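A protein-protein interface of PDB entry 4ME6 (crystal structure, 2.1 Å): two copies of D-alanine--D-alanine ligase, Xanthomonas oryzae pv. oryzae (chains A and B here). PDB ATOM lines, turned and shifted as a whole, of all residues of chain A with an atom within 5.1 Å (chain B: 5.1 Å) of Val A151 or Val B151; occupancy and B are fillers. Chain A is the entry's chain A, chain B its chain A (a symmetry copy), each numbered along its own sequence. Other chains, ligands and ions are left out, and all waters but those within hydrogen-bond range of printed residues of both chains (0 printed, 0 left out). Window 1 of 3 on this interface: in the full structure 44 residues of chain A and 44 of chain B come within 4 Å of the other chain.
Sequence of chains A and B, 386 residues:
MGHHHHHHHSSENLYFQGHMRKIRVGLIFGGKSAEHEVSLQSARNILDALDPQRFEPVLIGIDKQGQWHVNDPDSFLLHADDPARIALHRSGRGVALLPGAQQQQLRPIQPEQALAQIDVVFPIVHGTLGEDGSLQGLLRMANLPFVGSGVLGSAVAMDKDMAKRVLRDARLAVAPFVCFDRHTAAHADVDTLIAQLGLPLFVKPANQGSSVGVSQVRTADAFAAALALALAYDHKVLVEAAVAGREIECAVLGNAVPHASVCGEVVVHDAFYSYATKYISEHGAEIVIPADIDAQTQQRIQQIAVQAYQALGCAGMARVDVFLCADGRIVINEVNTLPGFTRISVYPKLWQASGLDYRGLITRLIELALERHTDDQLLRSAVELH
Asp A132 touches Val B151.
Ser A134 touches Val B151 (OG to CG2, 3.99 Å).
Val A151 touches Asp B132.
OG of Ser B134 touches CG2 of Val A151, at 3.99 Å.
CG1 of Val A151 touches CG1 of Val B151, at 3.6 Å.
Ala B155 touches Leu A152 (C to CD1, 3.7 Å).
CD1 of Leu A152 touches N of Val B156, at 3.8 Å.
CD1 of Leu B152 touches C of Ala A155, at 3.7 Å.
N of Val A156 touches CD1 of Leu B152, at 3.8 Å.
Of the printed residues of chain B, Ser A134 touches Gly B137 (3.3 Å), Arg B140 (2.9 Å) and Val B151 (3.99 Å).
Printed residues of chain B within 4 Å of Val A151: Asp B132, Ser B134 and Val B151.
Printed residues of chain A within 4 Å of Ser B134: Gly A137 (3.3 Å), Arg A140 (2.9 Å) and Val A151 (3.99 Å).
Of the printed residues of chain A, Val B151 touches Asp A132, Ser A134 and Val A151.
Of the printed residues of chain A, Leu B152 touches Ala A155 (3.7 Å) and Val A156 (3.8 Å).
The nearest printed residue of chain B that does not touch Val A151 is Gly B133 (4.01 Å).
OD1 of Asp A132 is in hydrogen-bond range of OG of Ser A134.
OG of Ser B134 lies within hydrogen-bond range of OD1 of Asp B132.
Asp A132 touches Val B151, and with the chains exchanged Val A151 touches Asp B132.
Ser A134 touches Gly B137, and with the chains exchanged Gly A137 touches Ser B134.
Ser A134 touches Arg B140, and with the chains exchanged Arg A140 touches Ser B134.
Ser A134 touches Val B151, and with the chains exchanged Val A151 touches Ser B134.
Of the 15 pairs that touch across the chains among the printed residues, 15 have their exchanged pair printed and touching as well.
OD2 of Asp A132 lies within salt-bridge range of NH2 of Arg B140 (3.1 Å).
The side-chain hydroxyl (OG) of Ser A134 sits at hydrogen-bond distance from the guanidinium group (NE) of Arg B140.
OD2 of Asp B132 is in salt-bridge range of NH2 of Arg A140 (3.1 Å).
The guanidinium group of Arg A140 sits at hydrogen-bond distance from the side-chain hydroxyl of Ser B134 (2.9 Å).
O of Ser A134 lies close to O of Gly B137 (3.3 Å).
O of Gly A137 sits close to O of Ser B134, at 3.3 Å.
Hydrophobic or aromatic side chains of chain B that line the printed part of chain A: Val B151, Leu B152, Ala B155 and Val B156.
Among the printed residues, 15 pairs touch across the chains.
Among the printed residues, Asp or Glu carboxylates within 4 Å of a Lys or Arg side-chain nitrogen of the other chain: Asp A132 with Arg B140 and Arg A140 with Asp B132.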
ATOM      1  N   ASP A 132       7.642  20.685  20.214  1.00  0.00           N
ATOM      2  CA  ASP A 132       8.110  22.050  19.995  1.00  0.00           C
ATOM      3  C   ASP A 132       8.211  22.857  21.272  1.00  0.00           C
ATOM      4  O   ASP A 132       8.440  24.043  21.210  1.00  0.00           O
ATOM      5  CB  ASP A 132       7.270  22.792  18.947  1.00  0.00           C
ATOM      6  CG  ASP A 132       5.898  23.196  19.429  1.00  0.00           C
ATOM      7  OD1 ASP A 132       5.504  22.986  20.605  1.00  0.00           O
ATOM      8  OD2 ASP A 132       5.133  23.736  18.589  1.00  0.00           O
ATOM      9  N   GLY A 133       7.969  22.219  22.418  1.00  0.00           N
ATOM     10  CA  GLY A 133       8.092  22.892  23.697  1.00  0.00           C
ATOM     11  C   GLY A 133       6.766  23.163  24.335  1.00  0.00           C
ATOM     12  O   GLY A 133       6.740  23.527  25.497  1.00  0.00           O
ATOM     13  N   SER A 134       5.681  23.040  23.574  1.00  0.00           N
ATOM     14  CA  SER A 134       4.368  23.351  24.056  1.00  0.00           C
ATOM     15  C   SER A 134       3.977  22.362  25.130  1.00  0.00           C
ATOM     16  O   SER A 134       3.504  22.785  26.155  1.00  0.00           O
ATOM     17  CB  SER A 134       3.290  23.316  22.969  1.00  0.00           C
ATOM     18  OG  SER A 134       3.636  24.146  21.859  1.00  0.00           O
ATOM     19  N   GLN A 136       5.960  20.372  26.779  1.00  0.00           N
ATOM     20  CA  GLN A 136       6.900  20.555  27.821  1.00  0.00           C
ATOM     21  C   GLN A 136       6.484  21.739  28.724  1.00  0.00           C
ATOM     22  O   GLN A 136       6.639  21.680  29.952  1.00  0.00           O
ATOM     23  CB  GLN A 136       8.322  20.772  27.248  1.00  0.00           C
ATOM     24  CG  GLN A 136       8.944  19.627  26.491  1.00  0.00           C
ATOM     25  CD  GLN A 136       8.296  19.274  25.182  1.00  0.00           C
ATOM     26  OE1 GLN A 136       7.712  20.115  24.486  1.00  0.00           O
ATOM     27  NE2 GLN A 136       8.433  18.056  24.819  1.00  0.00           N
ATOM     28  N   GLY A 137       5.948  22.806  28.128  1.00  0.00           N
ATOM     29  CA  GLY A 137       5.505  23.916  28.923  1.00  0.00           C
ATOM     30  C   GLY A 137       4.290  23.586  29.812  1.00  0.00           C
ATOM     31  O   GLY A 137       4.216  24.085  30.961  1.00  0.00           O
ATOM     32  N   ARG A 140       5.710  21.634  32.787  1.00  0.00           N
ATOM     33  CA  ARG A 140       6.222  22.604  33.748  1.00  0.00           C
ATOM     34  C   ARG A 140       5.173  23.318  34.532  1.00  0.00           C
ATOM     35  O   ARG A 140       5.364  23.597  35.719  1.00  0.00           O
ATOM     36  CB  ARG A 140       7.058  23.655  33.049  1.00  0.00           C
ATOM     37  CG  ARG A 140       8.463  23.181  32.868  1.00  0.00           C
ATOM     38  CD  ARG A 140       9.262  24.100  31.993  1.00  0.00           C
ATOM     39  NE  ARG A 140       9.559  25.376  32.651  1.00  0.00           N
ATOM     40  CZ  ARG A 140      10.505  25.579  33.554  1.00  0.00           C
ATOM     41  NH1 ARG A 140      11.300  24.594  33.946  1.00  0.00           N
ATOM     42  NH2 ARG A 140      10.660  26.782  34.051  1.00  0.00           N
ATOM     43  N   SER A 149      14.221  17.235  26.575  1.00  0.00           N
ATOM     44  CA  SER A 149      14.549  18.633  26.619  1.00  0.00           C
ATOM     45  C   SER A 149      13.411  19.486  27.185  1.00  0.00           C
ATOM     46  O   SER A 149      12.244  19.176  27.052  1.00  0.00           O
ATOM     47  CB  SER A 149      14.964  19.114  25.243  1.00  0.00           C
ATOM     48  OG  SER A 149      16.084  18.373  24.776  1.00  0.00           O
ATOM     49  N   GLY A 150      13.775  20.521  27.886  1.00  0.00           N
ATOM     50  CA  GLY A 150      12.805  21.494  28.373  1.00  0.00           C
ATOM     51  C   GLY A 150      12.259  22.383  27.267  1.00  0.00           C
ATOM     52  O   GLY A 150      12.294  22.012  26.090  1.00  0.00           O
ATOM     53  N   VAL A 151      11.706  23.523  27.651  1.00  0.00           N
ATOM     54  CA  VAL A 151      10.910  24.298  26.706  1.00  0.00           C
ATOM     55  C   VAL A 151      11.817  24.886  25.639  1.00  0.00           C
ATOM     56  O   VAL A 151      11.549  24.753  24.443  1.00  0.00           O
ATOM     57  CB  VAL A 151      10.111  25.382  27.468  1.00  0.00           C
ATOM     58  CG1 VAL A 151       9.418  26.362  26.532  1.00  0.00           C
ATOM     59  CG2 VAL A 151       9.052  24.737  28.331  1.00  0.00           C
ATOM     60  N   LEU A 152      12.891  25.517  26.085  1.00  0.00           N
ATOM     61  CA  LEU A 152      13.790  26.205  25.234  1.00  0.00           C
ATOM     62  C   LEU A 152      14.484  25.258  24.291  1.00  0.00           C
ATOM     63  O   LEU A 152      14.492  25.520  23.091  1.00  0.00           O
ATOM     64  CB  LEU A 152      14.843  26.969  26.068  1.00  0.00           C
ATOM     65  CG  LEU A 152      15.977  27.725  25.323  1.00  0.00           C
ATOM     66  CD1 LEU A 152      15.475  28.742  24.324  1.00  0.00           C
ATOM     67  CD2 LEU A 152      16.903  28.369  26.332  1.00  0.00           C
ATOM     68  N   GLY A 153      15.073  24.170  24.824  1.00  0.00           N
ATOM     69  CA  GLY A 153      15.794  23.205  24.008  1.00  0.00           C
ATOM     70  C   GLY A 153      14.911  22.562  22.916  1.00  0.00           C
ATOM     71  O   GLY A 153      15.321  22.392  21.770  1.00  0.00           O
ATOM     72  N   SER A 154      13.692  22.270  23.281  1.00  0.00           N
ATOM     73  CA  SER A 154      12.745  21.673  22.370  1.00  0.00           C
ATOM     74  C   SER A 154      12.323  22.684  21.271  1.00  0.00           C
ATOM     75  O   SER A 154      12.364  22.356  20.124  1.00  0.00           O
ATOM     76  CB  SER A 154      11.517  21.158  23.139  1.00  0.00           C
ATOM     77  OG  SER A 154      11.865  20.211  24.178  1.00  0.00           O
ATOM     78  N   ALA A 155      12.013  23.910  21.669  1.00  0.00           N
ATOM     79  CA  ALA A 155      11.556  24.962  20.762  1.00  0.00           C
ATOM     80  C   ALA A 155      12.657  25.265  19.779  1.00  0.00           C
ATOM     81  O   ALA A 155      12.397  25.330  18.605  1.00  0.00           O
ATOM     82  CB  ALA A 155      11.209  26.209  21.525  1.00  0.00           C
ATOM     83  N   VAL A 156      13.882  25.441  20.274  1.00  0.00           N
ATOM     84  CA  VAL A 156      15.010  25.770  19.414  1.00  0.00           C
ATOM     85  C   VAL A 156      15.354  24.646  18.408  1.00  0.00           C
ATOM     86  O   VAL A 156      15.551  24.897  17.198  1.00  0.00           O
ATOM     87  CB  VAL A 156      16.215  26.155  20.218  1.00  0.00           C
ATOM     88  CG1 VAL A 156      17.356  26.434  19.278  1.00  0.00           C
ATOM     89  CG2 VAL A 156      15.962  27.443  20.962  1.00  0.00           C
ATOM     90  N   ASP B 132       8.635  32.456  30.173  1.00  0.00           N
ATOM     91  CA  ASP B 132       9.698  31.683  29.539  1.00  0.00           C
ATOM     92  C   ASP B 132       9.190  30.719  28.490  1.00  0.00           C
ATOM     93  O   ASP B 132       9.951  29.914  28.002  1.00  0.00           O
ATOM     94  CB  ASP B 132      10.580  30.957  30.564  1.00  0.00           C
ATOM     95  CG  ASP B 132       9.918  29.766  31.215  1.00  0.00           C
ATOM     96  OD1 ASP B 132       8.764  29.378  30.901  1.00  0.00           O
ATOM     97  OD2 ASP B 132      10.561  29.180  32.123  1.00  0.00           O
ATOM     98  N   GLY B 133       7.887  30.760  28.203  1.00  0.00           N
ATOM     99  CA  GLY B 133       7.314  29.912  27.176  1.00  0.00           C
ATOM    100  C   GLY B 133       6.480  28.806  27.739  1.00  0.00           C
ATOM    101  O   GLY B 133       5.776  28.160  26.983  1.00  0.00           O
ATOM    102  N   SER B 134       6.592  28.553  29.041  1.00  0.00           N
ATOM    103  CA  SER B 134       5.903  27.468  29.673  1.00  0.00           C
ATOM    104  C   SER B 134       4.415  27.731  29.647  1.00  0.00           C
ATOM    105  O   SER B 134       3.683  26.841  29.293  1.00  0.00           O
ATOM    106  CB  SER B 134       6.315  27.245  31.133  1.00  0.00           C
ATOM    107  OG  SER B 134       7.730  27.096  31.262  1.00  0.00           O
ATOM    108  N   GLN B 136       2.838  29.877  27.772  1.00  0.00           N
ATOM    109  CA  GLN B 136       2.488  29.922  26.401  1.00  0.00           C
ATOM    110  C   GLN B 136       2.273  28.494  25.850  1.00  0.00           C
ATOM    111  O   GLN B 136       1.361  28.261  25.042  1.00  0.00           O
ATOM    112  CB  GLN B 136       3.567  30.673  25.581  1.00  0.00           C
ATOM    113  CG  GLN B 136       3.768  32.136  25.880  1.00  0.00           C
ATOM    114  CD  GLN B 136       4.339  32.460  27.232  1.00  0.00           C
ATOM    115  OE1 GLN B 136       5.100  31.686  27.831  1.00  0.00           O
ATOM    116  NE2 GLN B 136       4.022  33.608  27.696  1.00  0.00           N
ATOM    117  N   GLY B 137       3.094  27.538  26.287  1.00  0.00           N
ATOM    118  CA  GLY B 137       2.911  26.186  25.840  1.00  0.00           C
ATOM    119  C   GLY B 137       1.608  25.542  26.352  1.00  0.00           C
ATOM    120  O   GLY B 137       0.968  24.767  25.600  1.00  0.00           O
ATOM    121  N   ARG B 140      -1.170  26.969  24.133  1.00  0.00           N
ATOM    122  CA  ARG B 140      -1.198  26.186  22.904  1.00  0.00           C
ATOM    123  C   ARG B 140      -1.808  24.831  23.042  1.00  0.00           C
ATOM    124  O   ARG B 140      -2.494  24.361  22.131  1.00  0.00           O
ATOM    125  CB  ARG B 140       0.201  25.999  22.357  1.00  0.00           C
ATOM    126  CG  ARG B 140       0.608  27.174  21.530  1.00  0.00           C
ATOM    127  CD  ARG B 140       2.059  27.125  21.154  1.00  0.00           C
ATOM    128  NE  ARG B 140       2.342  26.074  20.171  1.00  0.00           N
ATOM    129  CZ  ARG B 140       2.112  26.147  18.870  1.00  0.00           C
ATOM    130  NH1 ARG B 140       1.586  27.236  18.329  1.00  0.00           N
ATOM    131  NH2 ARG B 140       2.428  25.126  18.111  1.00  0.00           N
ATOM    132  N   SER B 149       4.392  36.809  22.512  1.00  0.00           N
ATOM    133  CA  SER B 149       5.220  35.858  21.824  1.00  0.00           C
ATOM    134  C   SER B 149       4.820  34.410  22.115  1.00  0.00           C
ATOM    135  O   SER B 149       4.323  34.077  23.173  1.00  0.00           O
ATOM    136  CB  SER B 149       6.678  36.102  22.157  1.00  0.00           C
ATOM    137  OG  SER B 149       7.057  37.422  21.791  1.00  0.00           O
ATOM    138  N   GLY B 150       4.967  33.573  21.129  1.00  0.00           N
ATOM    139  CA  GLY B 150       4.753  32.142  21.302  1.00  0.00           C
ATOM    140  C   GLY B 150       5.864  31.472  22.092  1.00  0.00           C
ATOM    141  O   GLY B 150       6.578  32.133  22.852  1.00  0.00           O
ATOM    142  N   VAL B 151       5.971  30.159  21.958  1.00  0.00           N
ATOM    143  CA  VAL B 151       6.807  29.400  22.879  1.00  0.00           C
ATOM    144  C   VAL B 151       8.269  29.728  22.628  1.00  0.00           C
ATOM    145  O   VAL B 151       9.012  30.044  23.561  1.00  0.00           O
ATOM    146  CB  VAL B 151       6.504  27.890  22.731  1.00  0.00           C
ATOM    147  CG1 VAL B 151       7.481  27.019  23.509  1.00  0.00           C
ATOM    148  CG2 VAL B 151       5.112  27.587  23.233  1.00  0.00           C
ATOM    149  N   LEU B 152       8.661  29.663  21.366  1.00  0.00           N
ATOM    150  CA  LEU B 152      10.008  29.844  20.966  1.00  0.00           C
ATOM    151  C   LEU B 152      10.483  31.242  21.259  1.00  0.00           C
ATOM    152  O   LEU B 152      11.540  31.393  21.866  1.00  0.00           O
ATOM    153  CB  LEU B 152      10.166  29.548  19.458  1.00  0.00           C
ATOM    154  CG  LEU B 152      11.556  29.768  18.799  1.00  0.00           C
ATOM    155  CD1 LEU B 152      12.671  28.988  19.457  1.00  0.00           C
ATOM    156  CD2 LEU B 152      11.471  29.449  17.322  1.00  0.00           C
ATOM    157  N   GLY B 153       9.717  32.263  20.824  1.00  0.00           N
ATOM    158  CA  GLY B 153      10.097  33.653  21.029  1.00  0.00           C
ATOM    159  C   GLY B 153      10.261  34.018  22.520  1.00  0.00           C
ATOM    160  O   GLY B 153      11.198  34.708  22.917  1.00  0.00           O
ATOM    161  N   SER B 154       9.377  33.496  23.326  1.00  0.00           N
ATOM    162  CA  SER B 154       9.404  33.738  24.749  1.00  0.00           C
ATOM    163  C   SER B 154      10.622  33.035  25.405  1.00  0.00           C
ATOM    164  O   SER B 154      11.339  33.656  26.131  1.00  0.00           O
ATOM    165  CB  SER B 154       8.090  33.270  25.395  1.00  0.00           C
ATOM    166  OG  SER B 154       6.924  33.902  24.811  1.00  0.00           O
ATOM    167  N   ALA B 155      10.853  31.778  25.051  1.00  0.00           N
ATOM    168  CA  ALA B 155      11.933  30.967  25.611  1.00  0.00           C
ATOM    169  C   ALA B 155      13.251  31.600  25.247  1.00  0.00           C
ATOM    170  O   ALA B 155      14.085  31.756  26.102  1.00  0.00           O
ATOM    171  CB  ALA B 155      11.883  29.567  25.069  1.00  0.00           C
ATOM    172  N   VAL B 156      13.421  31.963  23.975  1.00  0.00           N
ATOM    173  CA  VAL B 156      14.670  32.553  23.513  1.00  0.00           C
ATOM    174  C   VAL B 156      14.968  33.926  24.161  1.00  0.00           C
ATOM    175  O   VAL B 156      16.098  34.187  24.633  1.00  0.00           O
ATOM    176  CB  VAL B 156      14.707  32.648  22.017  1.00  0.00           C
ATOM    177  CG1 VAL B 156      15.995  33.308  21.607  1.00  0.00           C
ATOM    178  CG2 VAL B 156      14.728  31.270  21.404  1.00  0.00           C
